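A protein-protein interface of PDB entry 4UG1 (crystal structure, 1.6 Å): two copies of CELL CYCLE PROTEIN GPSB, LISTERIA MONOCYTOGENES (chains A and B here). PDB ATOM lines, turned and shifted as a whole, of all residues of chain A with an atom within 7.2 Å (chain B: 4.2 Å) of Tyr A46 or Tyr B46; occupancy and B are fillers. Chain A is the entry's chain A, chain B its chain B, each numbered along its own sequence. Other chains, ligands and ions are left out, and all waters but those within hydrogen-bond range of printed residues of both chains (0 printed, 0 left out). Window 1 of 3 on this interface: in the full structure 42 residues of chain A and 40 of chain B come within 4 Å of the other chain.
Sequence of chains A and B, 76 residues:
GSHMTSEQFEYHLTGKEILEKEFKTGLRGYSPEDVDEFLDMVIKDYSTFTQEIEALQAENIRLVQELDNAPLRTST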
ATOM      1  N   TYR A  11      -0.740 -17.605 -25.547  1.00  0.00           N
ATOM      2  CA  TYR A  11      -0.723 -17.813 -24.095  1.00  0.00           C
ATOM      3  C   TYR A  11      -0.346 -16.549 -23.344  1.00  0.00           C
ATOM      4  O   TYR A  11       0.460 -15.751 -23.816  1.00  0.00           O
ATOM      5  CB  TYR A  11       0.237 -18.941 -23.732  1.00  0.00           C
ATOM      6  CG  TYR A  11      -0.222 -20.261 -24.299  1.00  0.00           C
ATOM      7  CD1 TYR A  11      -1.124 -21.053 -23.601  1.00  0.00           C
ATOM      8  CD2 TYR A  11       0.208 -20.693 -25.543  1.00  0.00           C
ATOM      9  CE1 TYR A  11      -1.568 -22.250 -24.111  1.00  0.00           C
ATOM     10  CE2 TYR A  11      -0.232 -21.898 -26.061  1.00  0.00           C
ATOM     11  CZ  TYR A  11      -1.122 -22.665 -25.333  1.00  0.00           C
ATOM     12  OH  TYR A  11      -1.584 -23.858 -25.819  1.00  0.00           O
ATOM     13  N   HIS A  12      -0.931 -16.380 -22.164  1.00  0.00           N
ATOM     14  CA  HIS A  12      -0.707 -15.191 -21.342  1.00  0.00           C
ATOM     15  C   HIS A  12       0.511 -15.299 -20.432  1.00  0.00           C
ATOM     16  O   HIS A  12       1.230 -14.312 -20.209  1.00  0.00           O
ATOM     17  CB  HIS A  12      -1.946 -14.907 -20.484  1.00  0.00           C
ATOM     18  CG  HIS A  12      -3.146 -14.499 -21.272  1.00  0.00           C
ATOM     19  ND1 HIS A  12      -4.189 -15.360 -21.542  1.00  0.00           N
ATOM     20  CD2 HIS A  12      -3.469 -13.320 -21.855  1.00  0.00           C
ATOM     21  CE1 HIS A  12      -5.100 -14.727 -22.260  1.00  0.00           C
ATOM     22  NE2 HIS A  12      -4.691 -13.488 -22.457  1.00  0.00           N
ATOM     23  N   LEU A  13       0.728 -16.490 -19.890  1.00  0.00           N
ATOM     24  CA  LEU A  13       1.756 -16.696 -18.885  1.00  0.00           C
ATOM     25  C   LEU A  13       2.675 -17.856 -19.242  1.00  0.00           C
ATOM     26  O   LEU A  13       2.364 -18.684 -20.088  1.00  0.00           O
ATOM     27  CB  LEU A  13       1.114 -16.958 -17.513  1.00  0.00           C
ATOM     28  CG  LEU A  13       0.344 -15.801 -16.872  1.00  0.00           C
ATOM     29  CD1 LEU A  13      -0.510 -16.291 -15.713  1.00  0.00           C
ATOM     30  CD2 LEU A  13       1.314 -14.746 -16.371  1.00  0.00           C
ATOM     31  N   THR A  14       3.822 -17.880 -18.586  1.00  0.00           N
ATOM     32  CA  THR A  14       4.712 -19.023 -18.607  1.00  0.00           C
ATOM     33  C   THR A  14       4.836 -19.511 -17.174  1.00  0.00           C
ATOM     34  O   THR A  14       4.538 -18.771 -16.239  1.00  0.00           O
ATOM     35  CB  THR A  14       6.093 -18.663 -19.157  1.00  0.00           C
ATOM     36  OG1 THR A  14       6.713 -17.714 -18.278  1.00  0.00           O
ATOM     37  CG2 THR A  14       5.961 -18.055 -20.548  1.00  0.00           C
ATOM     38  N   GLY A  15       5.276 -20.751 -16.996  1.00  0.00           N
ATOM     39  CA  GLY A  15       5.513 -21.265 -15.659  1.00  0.00           C
ATOM     40  C   GLY A  15       6.485 -20.381 -14.897  1.00  0.00           C
ATOM     41  O   GLY A  15       6.337 -20.151 -13.695  1.00  0.00           O
ATOM     42  N   LYS A  16       7.481 -19.864 -15.610  1.00  0.00           N
ATOM     43  CA  LYS A  16       8.482 -19.004 -14.996  1.00  0.00           C
ATOM     44  C   LYS A  16       7.853 -17.731 -14.434  1.00  0.00           C
ATOM     45  O   LYS A  16       8.168 -17.314 -13.320  1.00  0.00           O
ATOM     46  CB  LYS A  16       9.570 -18.656 -16.006  1.00  0.00           C
ATOM     47  CG  LYS A  16      10.712 -17.827 -15.442  1.00  0.00           C
ATOM     48  CD  LYS A  16      11.850 -17.722 -16.458  1.00  0.00           C
ATOM     49  CE  LYS A  16      12.999 -16.873 -15.946  1.00  0.00           C
ATOM     50  NZ  LYS A  16      12.555 -15.492 -15.606  1.00  0.00           N
ATOM     51  N   ILE A  18       4.852 -17.407 -13.428  1.00  0.00           N
ATOM     52  CA  ILE A  18       4.047 -17.733 -12.267  1.00  0.00           C
ATOM     53  C   ILE A  18       4.945 -17.981 -11.050  1.00  0.00           C
ATOM     54  O   ILE A  18       4.640 -17.521  -9.954  1.00  0.00           O
ATOM     55  CB  ILE A  18       3.140 -18.940 -12.552  1.00  0.00           C
ATOM     56  CG1 ILE A  18       2.192 -18.598 -13.704  1.00  0.00           C
ATOM     57  CG2 ILE A  18       2.347 -19.315 -11.305  1.00  0.00           C
ATOM     58  CD1 ILE A  18       1.451 -19.805 -14.289  1.00  0.00           C
ATOM     59  N   PHE A  38      -1.871 -23.595  -4.087  1.00  0.00           N
ATOM     60  CA  PHE A  38      -2.666 -23.721  -5.303  1.00  0.00           C
ATOM     61  C   PHE A  38      -1.824 -23.436  -6.551  1.00  0.00           C
ATOM     62  O   PHE A  38      -1.905 -24.163  -7.545  1.00  0.00           O
ATOM     63  CB  PHE A  38      -3.864 -22.772  -5.209  1.00  0.00           C
ATOM     64  CG  PHE A  38      -4.996 -23.093  -6.151  1.00  0.00           C
ATOM     65  CD1 PHE A  38      -5.812 -24.185  -5.924  1.00  0.00           C
ATOM     66  CD2 PHE A  38      -5.261 -22.269  -7.232  1.00  0.00           C
ATOM     67  CE1 PHE A  38      -6.880 -24.470  -6.775  1.00  0.00           C
ATOM     68  CE2 PHE A  38      -6.327 -22.538  -8.079  1.00  0.00           C
ATOM     69  CZ  PHE A  38      -7.135 -23.642  -7.849  1.00  0.00           C
ATOM     70  N   LEU A  39      -1.015 -22.381  -6.513  1.00  0.00           N
ATOM     71  CA  LEU A  39      -0.170 -22.037  -7.656  1.00  0.00           C
ATOM     72  C   LEU A  39       0.914 -23.078  -7.917  1.00  0.00           C
ATOM     73  O   LEU A  39       1.366 -23.226  -9.052  1.00  0.00           O
ATOM     74  CB  LEU A  39       0.488 -20.669  -7.453  1.00  0.00           C
ATOM     75  CG  LEU A  39      -0.430 -19.456  -7.569  1.00  0.00           C
ATOM     76  CD1 LEU A  39       0.370 -18.193  -7.305  1.00  0.00           C
ATOM     77  CD2 LEU A  39      -1.109 -19.374  -8.933  1.00  0.00           C
ATOM     78  N   ASP A  40       1.361 -23.760  -6.869  1.00  0.00           N
ATOM     79  CA  ASP A  40       2.322 -24.847  -7.034  1.00  0.00           C
ATOM     80  C   ASP A  40       1.752 -25.885  -8.007  1.00  0.00           C
ATOM     81  O   ASP A  40       2.460 -26.377  -8.895  1.00  0.00           O
ATOM     82  CB  ASP A  40       2.656 -25.491  -5.683  1.00  0.00           C
ATOM     83  CG  ASP A  40       3.783 -26.485  -5.781  1.00  0.00           C
ATOM     84  OD1 ASP A  40       4.828 -26.134  -6.364  1.00  0.00           O
ATOM     85  OD2 ASP A  40       3.621 -27.619  -5.289  1.00  0.00           O
ATOM     86  N   MET A  41       0.473 -26.211  -7.836  1.00  0.00           N
ATOM     87  CA  MET A  41      -0.198 -27.163  -8.725  1.00  0.00           C
ATOM     88  C   MET A  41      -0.340 -26.591 -10.131  1.00  0.00           C
ATOM     89  O   MET A  41      -0.165 -27.300 -11.111  1.00  0.00           O
ATOM     90  CB  MET A  41      -1.574 -27.545  -8.174  1.00  0.00           C
ATOM     91  CG  MET A  41      -1.507 -28.457  -6.972  1.00  0.00           C
ATOM     92  SD  MET A  41      -3.112 -29.130  -6.497  1.00  0.00           S
ATOM     93  CE  MET A  41      -3.860 -27.654  -5.814  1.00  0.00           C
ATOM     94  N   VAL A  42      -0.654 -25.304 -10.227  1.00  0.00           N
ATOM     95  CA  VAL A  42      -0.761 -24.643 -11.524  1.00  0.00           C
ATOM     96  C   VAL A  42       0.546 -24.711 -12.308  1.00  0.00           C
ATOM     97  O   VAL A  42       0.546 -25.021 -13.501  1.00  0.00           O
ATOM     98  CB  VAL A  42      -1.175 -23.183 -11.335  1.00  0.00           C
ATOM     99  CG1 VAL A  42      -1.046 -22.407 -12.645  1.00  0.00           C
ATOM    100  CG2 VAL A  42      -2.584 -23.124 -10.802  1.00  0.00           C
ATOM    101  N   ILE A  43       1.663 -24.432 -11.636  1.00  0.00           N
ATOM    102  CA  ILE A  43       2.971 -24.456 -12.282  1.00  0.00           C
ATOM    103  C   ILE A  43       3.277 -25.869 -12.775  1.00  0.00           C
ATOM    104  O   ILE A  43       3.758 -26.047 -13.896  1.00  0.00           O
ATOM    105  CB  ILE A  43       4.078 -23.963 -11.338  1.00  0.00           C
ATOM    106  CG1 ILE A  43       3.842 -22.494 -10.987  1.00  0.00           C
ATOM    107  CG2 ILE A  43       5.450 -24.123 -11.999  1.00  0.00           C
ATOM    108  CD1 ILE A  43       4.606 -22.023  -9.766  1.00  0.00           C
ATOM    109  N   LYS A  44       2.990 -26.865 -11.938  1.00  0.00           N
ATOM    110  CA  LYS A  44       3.144 -28.266 -12.336  1.00  0.00           C
ATOM    111  C   LYS A  44       2.322 -28.552 -13.596  1.00  0.00           C
ATOM    112  O   LYS A  44       2.809 -29.199 -14.527  1.00  0.00           O
ATOM    113  CB  LYS A  44       2.719 -29.207 -11.204  1.00  0.00           C
ATOM    114  CG  LYS A  44       3.738 -29.382 -10.085  1.00  0.00           C
ATOM    115  CD  LYS A  44       3.181 -30.303  -9.005  1.00  0.00           C
ATOM    116  CE  LYS A  44       3.823 -30.056  -7.649  1.00  0.00           C
ATOM    117  NZ  LYS A  44       5.297 -29.960  -7.738  1.00  0.00           N
ATOM    118  N   ASP A  45       1.078 -28.075 -13.625  1.00  0.00           N
ATOM    119  CA  ASP A  45       0.222 -28.316 -14.793  1.00  0.00           C
ATOM    120  C   ASP A  45       0.758 -27.612 -16.037  1.00  0.00           C
ATOM    121  O   ASP A  45       0.725 -28.188 -17.112  1.00  0.00           O
ATOM    122  CB  ASP A  45      -1.226 -27.887 -14.537  1.00  0.00           C
ATOM    123  CG  ASP A  45      -1.983 -28.876 -13.660  1.00  0.00           C
ATOM    124  OD1 ASP A  45      -1.500 -30.019 -13.444  1.00  0.00           O
ATOM    125  OD2 ASP A  45      -3.087 -28.514 -13.193  1.00  0.00           O
ATOM    126  N   TYR A  46       1.255 -26.378 -15.908  1.00  0.00           N
ATOM    127  CA  TYR A  46       1.851 -25.709 -17.067  1.00  0.00           C
ATOM    128  C   TYR A  46       2.993 -26.554 -17.644  1.00  0.00           C
ATOM    129  O   TYR A  46       3.090 -26.713 -18.856  1.00  0.00           O
ATOM    130  CB  TYR A  46       2.371 -24.325 -16.697  1.00  0.00           C
ATOM    131  CG  TYR A  46       1.402 -23.180 -16.911  1.00  0.00           C
ATOM    132  CD1 TYR A  46       0.233 -23.079 -16.164  1.00  0.00           C
ATOM    133  CD2 TYR A  46       1.680 -22.182 -17.834  1.00  0.00           C
ATOM    134  CE1 TYR A  46      -0.646 -22.017 -16.346  1.00  0.00           C
ATOM    135  CE2 TYR A  46       0.827 -21.114 -18.015  1.00  0.00           C
ATOM    136  CZ  TYR A  46      -0.337 -21.041 -17.275  1.00  0.00           C
ATOM    137  OH  TYR A  46      -1.174 -19.964 -17.458  1.00  0.00           O
ATOM    138  N   SER A  47       3.840 -27.099 -16.770  1.00  0.00           N
ATOM    139  CA  SER A  47       4.951 -27.953 -17.190  1.00  0.00           C
ATOM    140  C   SER A  47       4.423 -29.192 -17.909  1.00  0.00           C
ATOM    141  O   SER A  47       4.899 -29.552 -18.988  1.00  0.00           O
ATOM    142  CB  SER A  47       5.807 -28.356 -15.989  1.00  0.00           C
ATOM    143  OG  SER A  47       6.878 -29.178 -16.413  1.00  0.00           O
ATOM    144  N   THR A  48       3.413 -29.819 -17.321  1.00  0.00           N
ATOM    145  CA  THR A  48       2.818 -31.021 -17.909  1.00  0.00           C
ATOM    146  C   THR A  48       2.134 -30.744 -19.247  1.00  0.00           C
ATOM    147  O   THR A  48       2.330 -31.494 -20.201  1.00  0.00           O
ATOM    148  CB  THR A  48       1.825 -31.654 -16.936  1.00  0.00           C
ATOM    149  OG1 THR A  48       2.520 -31.957 -15.728  1.00  0.00           O
ATOM    150  CG2 THR A  48       1.240 -32.947 -17.520  1.00  0.00           C
ATOM    151  N   PHE A  49       1.330 -29.679 -19.320  1.00  0.00           N
ATOM    152  CA  PHE A  49       0.746 -29.245 -20.596  1.00  0.00           C
ATOM    153  C   PHE A  49       1.823 -29.108 -21.676  1.00  0.00           C
ATOM    154  O   PHE A  49       1.660 -29.572 -22.804  1.00  0.00           O
ATOM    155  CB  PHE A  49       0.051 -27.887 -20.454  1.00  0.00           C
ATOM    156  CG  PHE A  49      -1.354 -27.935 -19.913  1.00  0.00           C
ATOM    157  CD1 PHE A  49      -2.316 -28.791 -20.437  1.00  0.00           C
ATOM    158  CD2 PHE A  49      -1.719 -27.057 -18.903  1.00  0.00           C
ATOM    159  CE1 PHE A  49      -3.610 -28.786 -19.955  1.00  0.00           C
ATOM    160  CE2 PHE A  49      -3.012 -27.047 -18.398  1.00  0.00           C
ATOM    161  CZ  PHE A  49      -3.963 -27.913 -18.919  1.00  0.00           C
ATOM    162  N   THR A  50       2.905 -28.426 -21.326  1.00  0.00           N
ATOM    163  CA  THR A  50       3.994 -28.175 -22.258  1.00  0.00           C
ATOM    164  C   THR A  50       4.621 -29.492 -22.712  1.00  0.00           C
ATOM    165  O   THR A  50       4.908 -29.689 -23.901  1.00  0.00           O
ATOM    166  CB  THR A  50       5.062 -27.259 -21.622  1.00  0.00           C
ATOM    167  OG1 THR A  50       4.469 -25.985 -21.327  1.00  0.00           O
ATOM    168  CG2 THR A  50       6.259 -27.063 -22.563  1.00  0.00           C
ATOM    169  N   GLN A  51       4.828 -30.401 -21.766  1.00  0.00           N
ATOM    170  CA  GLN A  51       5.415 -31.694 -22.086  1.00  0.00           C
ATOM    171  C   GLN A  51       4.493 -32.524 -22.968  1.00  0.00           C
ATOM    172  O   GLN A  51       4.962 -33.213 -23.876  1.00  0.00           O
ATOM    173  CB  GLN A  51       5.753 -32.465 -20.811  1.00  0.00           C
ATOM    174  CG  GLN A  51       6.855 -31.820 -19.987  1.00  0.00           C
ATOM    175  CD  GLN A  51       6.968 -32.404 -18.593  1.00  0.00           C
ATOM    176  OE1 GLN A  51       5.995 -32.923 -18.045  1.00  0.00           O
ATOM    177  NE2 GLN A  51       8.156 -32.324 -18.013  1.00  0.00           N
ATOM    178  N   GLU A  52       3.188 -32.493 -22.694  1.00  0.00           N
ATOM    179  CA  GLU A  52       2.267 -33.299 -23.483  1.00  0.00           C
ATOM    180  C   GLU A  52       2.147 -32.752 -24.897  1.00  0.00           C
ATOM    181  O   GLU A  52       2.061 -33.524 -25.863  1.00  0.00           O
ATOM    182  CB  GLU A  52       0.887 -33.388 -22.818  1.00  0.00           C
ATOM    183  CG  GLU A  52      -0.023 -34.356 -23.570  1.00  0.00           C
ATOM    184  CD  GLU A  52      -1.337 -34.670 -22.881  1.00  0.00           C
ATOM    185  OE1 GLU A  52      -1.792 -33.880 -22.017  1.00  0.00           O
ATOM    186  OE2 GLU A  52      -1.925 -35.724 -23.220  1.00  0.00           O
ATOM    187  N   LEU B  13      -5.298 -29.900 -11.749  1.00  0.00           N
ATOM    188  CA  LEU B  13      -6.448 -28.991 -11.728  1.00  0.00           C
ATOM    189  C   LEU B  13      -7.128 -28.885 -13.078  1.00  0.00           C
ATOM    190  O   LEU B  13      -6.504 -29.111 -14.123  1.00  0.00           O
ATOM    191  CB  LEU B  13      -6.016 -27.579 -11.304  1.00  0.00           C
ATOM    192  CG  LEU B  13      -5.470 -27.399  -9.891  1.00  0.00           C
ATOM    193  CD1 LEU B  13      -4.822 -26.013  -9.740  1.00  0.00           C
ATOM    194  CD2 LEU B  13      -6.564 -27.580  -8.844  1.00  0.00           C
ATOM    195  N   THR B  14      -8.408 -28.510 -13.041  1.00  0.00           N
ATOM    196  CA  THR B  14      -9.120 -28.034 -14.227  1.00  0.00           C
ATOM    197  C   THR B  14      -9.251 -26.508 -14.214  1.00  0.00           C
ATOM    198  O   THR B  14      -9.144 -25.870 -13.150  1.00  0.00           O
ATOM    199  CB  THR B  14     -10.530 -28.625 -14.329  1.00  0.00           C
ATOM    200  OG1 THR B  14     -11.328 -28.178 -13.218  1.00  0.00           O
ATOM    201  CG2 THR B  14     -10.487 -30.150 -14.326  1.00  0.00           C
ATOM    202  N   GLY B  15      -9.528 -25.937 -15.381  1.00  0.00           N
ATOM    203  CA  GLY B  15      -9.790 -24.515 -15.477  1.00  0.00           C
ATOM    204  C   GLY B  15     -10.993 -24.155 -14.630  1.00  0.00           C
ATOM    205  O   GLY B  15     -10.999 -23.114 -13.980  1.00  0.00           O
ATOM    206  N   ILE B  18     -10.098 -23.719 -11.113  1.00  0.00           N
ATOM    207  CA  ILE B  18      -9.355 -22.487 -10.863  1.00  0.00           C
ATOM    208  C   ILE B  18     -10.313 -21.284 -10.880  1.00  0.00           C
ATOM    209  O   ILE B  18     -10.166 -20.356 -10.080  1.00  0.00           O
ATOM    210  CB  ILE B  18      -8.208 -22.313 -11.879  1.00  0.00           C
ATOM    211  CG1 ILE B  18      -7.211 -23.469 -11.714  1.00  0.00           C
ATOM    212  CG2 ILE B  18      -7.520 -20.974 -11.685  1.00  0.00           C
ATOM    213  CD1 ILE B  18      -6.283 -23.629 -12.910  1.00  0.00           C
ATOM    214  N   VAL B  42      -4.437 -17.510 -16.106  1.00  0.00           N
ATOM    215  CA  VAL B  42      -4.232 -18.953 -15.953  1.00  0.00           C
ATOM    216  C   VAL B  42      -5.420 -19.749 -16.495  1.00  0.00           C
ATOM    217  O   VAL B  42      -5.246 -20.724 -17.233  1.00  0.00           O
ATOM    218  CB  VAL B  42      -3.996 -19.306 -14.473  1.00  0.00           C
ATOM    219  CG1 VAL B  42      -4.012 -20.813 -14.262  1.00  0.00           C
ATOM    220  CG2 VAL B  42      -2.681 -18.705 -13.986  1.00  0.00           C
ATOM    221  N   ILE B  43      -6.630 -19.319 -16.148  1.00  0.00           N
ATOM    222  CA  ILE B  43      -7.833 -20.002 -16.617  1.00  0.00           C
ATOM    223  C   ILE B  43      -7.894 -20.000 -18.146  1.00  0.00           C
ATOM    224  O   ILE B  43      -8.165 -21.021 -18.781  1.00  0.00           O
ATOM    225  CB  ILE B  43      -9.104 -19.345 -16.033  1.00  0.00           C
ATOM    226  CG1 ILE B  43      -9.177 -19.577 -14.525  1.00  0.00           C
ATOM    227  CG2 ILE B  43     -10.356 -19.896 -16.705  1.00  0.00           C
ATOM    228  CD1 ILE B  43     -10.007 -18.545 -13.792  1.00  0.00           C
ATOM    229  N   LYS B  44      -7.615 -18.850 -18.745  1.00  0.00           N
ATOM    230  CA  LYS B  44      -7.654 -18.747 -20.194  1.00  0.00           C
ATOM    231  C   LYS B  44      -6.560 -19.625 -20.812  1.00  0.00           C
ATOM    232  O   LYS B  44      -6.783 -20.273 -21.830  1.00  0.00           O
ATOM    233  CB  LYS B  44      -7.524 -17.281 -20.617  1.00  0.00           C
ATOM    234  CG  LYS B  44      -8.718 -16.434 -20.143  1.00  0.00           C
ATOM    235  CD  LYS B  44      -8.464 -14.924 -20.196  1.00  0.00           C
ATOM    236  CE  LYS B  44      -9.568 -14.162 -19.464  1.00  0.00           C
ATOM    237  NZ  LYS B  44      -9.435 -12.671 -19.564  1.00  0.00           N
ATOM    238  N   ASP B  45      -5.398 -19.687 -20.165  1.00  0.00           N
ATOM    239  CA  ASP B  45      -4.308 -20.523 -20.674  1.00  0.00           C
ATOM    240  C   ASP B  45      -4.624 -22.013 -20.589  1.00  0.00           C
ATOM    241  O   ASP B  45      -4.305 -22.756 -21.516  1.00  0.00           O
ATOM    242  CB  ASP B  45      -3.007 -20.247 -19.929  1.00  0.00           C
ATOM    243  CG  ASP B  45      -2.314 -18.967 -20.389  1.00  0.00           C
ATOM    244  OD1 ASP B  45      -2.731 -18.341 -21.391  1.00  0.00           O
ATOM    245  OD2 ASP B  45      -1.322 -18.592 -19.736  1.00  0.00           O
ATOM    246  N   TYR B  46      -5.223 -22.464 -19.490  1.00  0.00           N
ATOM    247  CA  TYR B  46      -5.651 -23.871 -19.382  1.00  0.00           C
ATOM    248  C   TYR B  46      -6.584 -24.245 -20.535  1.00  0.00           C
ATOM    249  O   TYR B  46      -6.459 -25.318 -21.134  1.00  0.00           O
ATOM    250  CB  TYR B  46      -6.370 -24.134 -18.064  1.00  0.00           C
ATOM    251  CG  TYR B  46      -5.528 -24.629 -16.913  1.00  0.00           C
ATOM    252  CD1 TYR B  46      -4.482 -23.853 -16.399  1.00  0.00           C
ATOM    253  CD2 TYR B  46      -5.814 -25.831 -16.302  1.00  0.00           C
ATOM    254  CE1 TYR B  46      -3.735 -24.291 -15.315  1.00  0.00           C
ATOM    255  CE2 TYR B  46      -5.072 -26.285 -15.210  1.00  0.00           C
ATOM    256  CZ  TYR B  46      -4.038 -25.509 -14.725  1.00  0.00           C
ATOM    257  OH  TYR B  46      -3.331 -25.944 -13.627  1.00  0.00           O
ATOM    258  N   SER B  47      -7.520 -23.356 -20.853  1.00  0.00           N
ATOM    259  CA  SER B  47      -8.439 -23.606 -21.953  1.00  0.00           C
ATOM    260  C   SER B  47      -7.696 -23.712 -23.290  1.00  0.00           C
ATOM    261  O   SER B  47      -7.991 -24.590 -24.107  1.00  0.00           O
ATOM    262  CB  SER B  47      -9.504 -22.508 -22.010  1.00  0.00           C
ATOM    263  OG  SER B  47     -10.448 -22.786 -23.030  1.00  0.00           O
ATOM    264  N   THR B  48      -6.729 -22.826 -23.511  1.00  0.00           N
ATOM    265  CA  THR B  48      -5.945 -22.846 -24.746  1.00  0.00           C
ATOM    266  C   THR B  48      -5.069 -24.102 -24.841  1.00  0.00           C
ATOM    267  O   THR B  48      -5.054 -24.761 -25.893  1.00  0.00           O
ATOM    268  CB  THR B  48      -5.082 -21.568 -24.863  1.00  0.00           C
ATOM    269  OG1 THR B  48      -5.938 -20.413 -24.783  1.00  0.00           O
ATOM    270  CG2 THR B  48      -4.337 -21.524 -26.197  1.00  0.00           C
ATOM    271  N   PHE B  49      -4.379 -24.443 -23.750  1.00  0.00           N
ATOM    272  CA  PHE B  49      -3.567 -25.671 -23.695  1.00  0.00           C
ATOM    273  C   PHE B  49      -4.425 -26.869 -24.056  1.00  0.00           C
ATOM    274  O   PHE B  49      -4.041 -27.732 -24.852  1.00  0.00           O
ATOM    275  CB  PHE B  49      -2.993 -25.906 -22.302  1.00  0.00           C
ATOM    276  CG  PHE B  49      -1.735 -25.135 -21.994  1.00  0.00           C
ATOM    277  CD1 PHE B  49      -0.632 -25.189 -22.818  1.00  0.00           C
ATOM    278  CD2 PHE B  49      -1.659 -24.386 -20.828  1.00  0.00           C
ATOM    279  CE1 PHE B  49       0.526 -24.496 -22.490  1.00  0.00           C
ATOM    280  CE2 PHE B  49      -0.511 -23.683 -20.498  1.00  0.00           C
ATOM    281  CZ  PHE B  49       0.577 -23.736 -21.322  1.00  0.00           C
ATOM    282  N   THR B  50      -5.592 -26.922 -23.427  1.00  0.00           N
ATOM    283  CA  THR B  50      -6.510 -28.043 -23.579  1.00  0.00           C
ATOM    284  C   THR B  50      -6.950 -28.176 -25.032  1.00  0.00           C
ATOM    285  O   THR B  50      -7.002 -29.289 -25.585  1.00  0.00           O
ATOM    286  CB  THR B  50      -7.728 -27.864 -22.659  1.00  0.00           C
ATOM    287  OG1 THR B  50      -7.285 -27.897 -21.297  1.00  0.00           O
ATOM    288  CG2 THR B  50      -8.761 -28.963 -22.880  1.00  0.00           C
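Of the 13 printed residues of chain B, 8 touch a printed residue of chain A. Printed residues of chain B that touch a printed residue of chain A: Leu B13, Ile B18, Val B42, Lys B44, Asp B45, Tyr B46, Thr B48 and Phe B49. Hydrophobic or aromatic side chains of chain B within 4 Å of the printed part of chain A: Leu B13, Ile B18, Val B42, Tyr B46 and Phe B49. Of the 22 printed residues of chain A, 9 touch a printed residue of chain B. Hydrophobic or aromatic side chains of chain A that line the printed part of chain B: Tyr A11, His A12, Leu A13, Phe A38, Met A41, Val A42, Tyr A46 and Phe A49. Along chain A the printed residues that touch a printed residue of chain B span positions 11 to 49. Among the printed residues, no Asp or Glu carboxylate lies within 4 Å of a Lys or Arg side-chain nitrogen of the other chain.
Of the printed residues of chain B, Phe A38 touches Leu B13 (3.7 Å) and Ile B18 (3.9 Å). Printed residues of chain B within 4 Å of Met A41: Leu B13. Tyr B46 touches just these residues of chain A: Val A42, Asp A45, Tyr A46 and Phe A49. The nearest printed residue of chain B that does not touch Tyr A46 is Ile B43 (5.6 Å). The nearest printed residue of chain A that does not touch Val B42 is Ile A18 (4.3 Å).
OG1 of Thr A50 sits at hydrogen-bond distance from O of Tyr A46 (2.9 Å). OG1 of Thr B48 sits at hydrogen-bond distance from O of Lys B44, 3.1 Å away. The side-chain hydroxyl (OG1) of Thr B50 sits at hydrogen-bond distance from the backbone carbonyl oxygen (O) of Tyr B46 (2.7 Å).
Val B42 touches its own counterpart, Val A42. Val A42 touches Tyr B46, and with the chains exchanged Tyr A46 touches Val B42. Tyr A46 touches its own counterpart, Tyr B46. Tyr A46 touches Phe B49, and with the chains exchanged Phe A49 touches Tyr B46. 13 positions are printed for both chains.
CA of Tyr A11 touches OD1 of Asp B45 (3.4 Å). CE1 of Tyr A11 touches CD1 of Phe B49, at 3.3 Å. His A12 touches Lys B44 (CE1 to CB, 3.9 Å). Leu B13 touches Phe A38 (CD2 to CE1, 3.7 Å). Leu B13 touches Met A41. Val A42 touches Leu B13 (CG2 to CD1, 3.8 Å). Val B42 touches Val A42. OH of Tyr A46 touches CA of Val B42, at 3.6 Å. Tyr A46 touches Phe B49. Tyr B46 touches Phe A49.
N of His A12 sits at hydrogen-bond distance from OD1 of Asp B45 (2.8 Å). The side-chain carboxylate (OD2) of Asp B45 lies within hydrogen-bond range of the backbone NH (N) of Leu A13 (2.9 Å). The backbone NH (N) of Leu B13 sits at hydrogen-bond distance from the side-chain carboxylate (OD2) of Asp A45, at 3.0 Å. The side-chain carboxylate of Asp A45 is in hydrogen-bond range of the side-chain hydroxyl of Tyr B46 (2.6 Å). OH of Tyr A46 sits at hydrogen-bond distance from OD2 of Asp B45 (2.7 Å).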
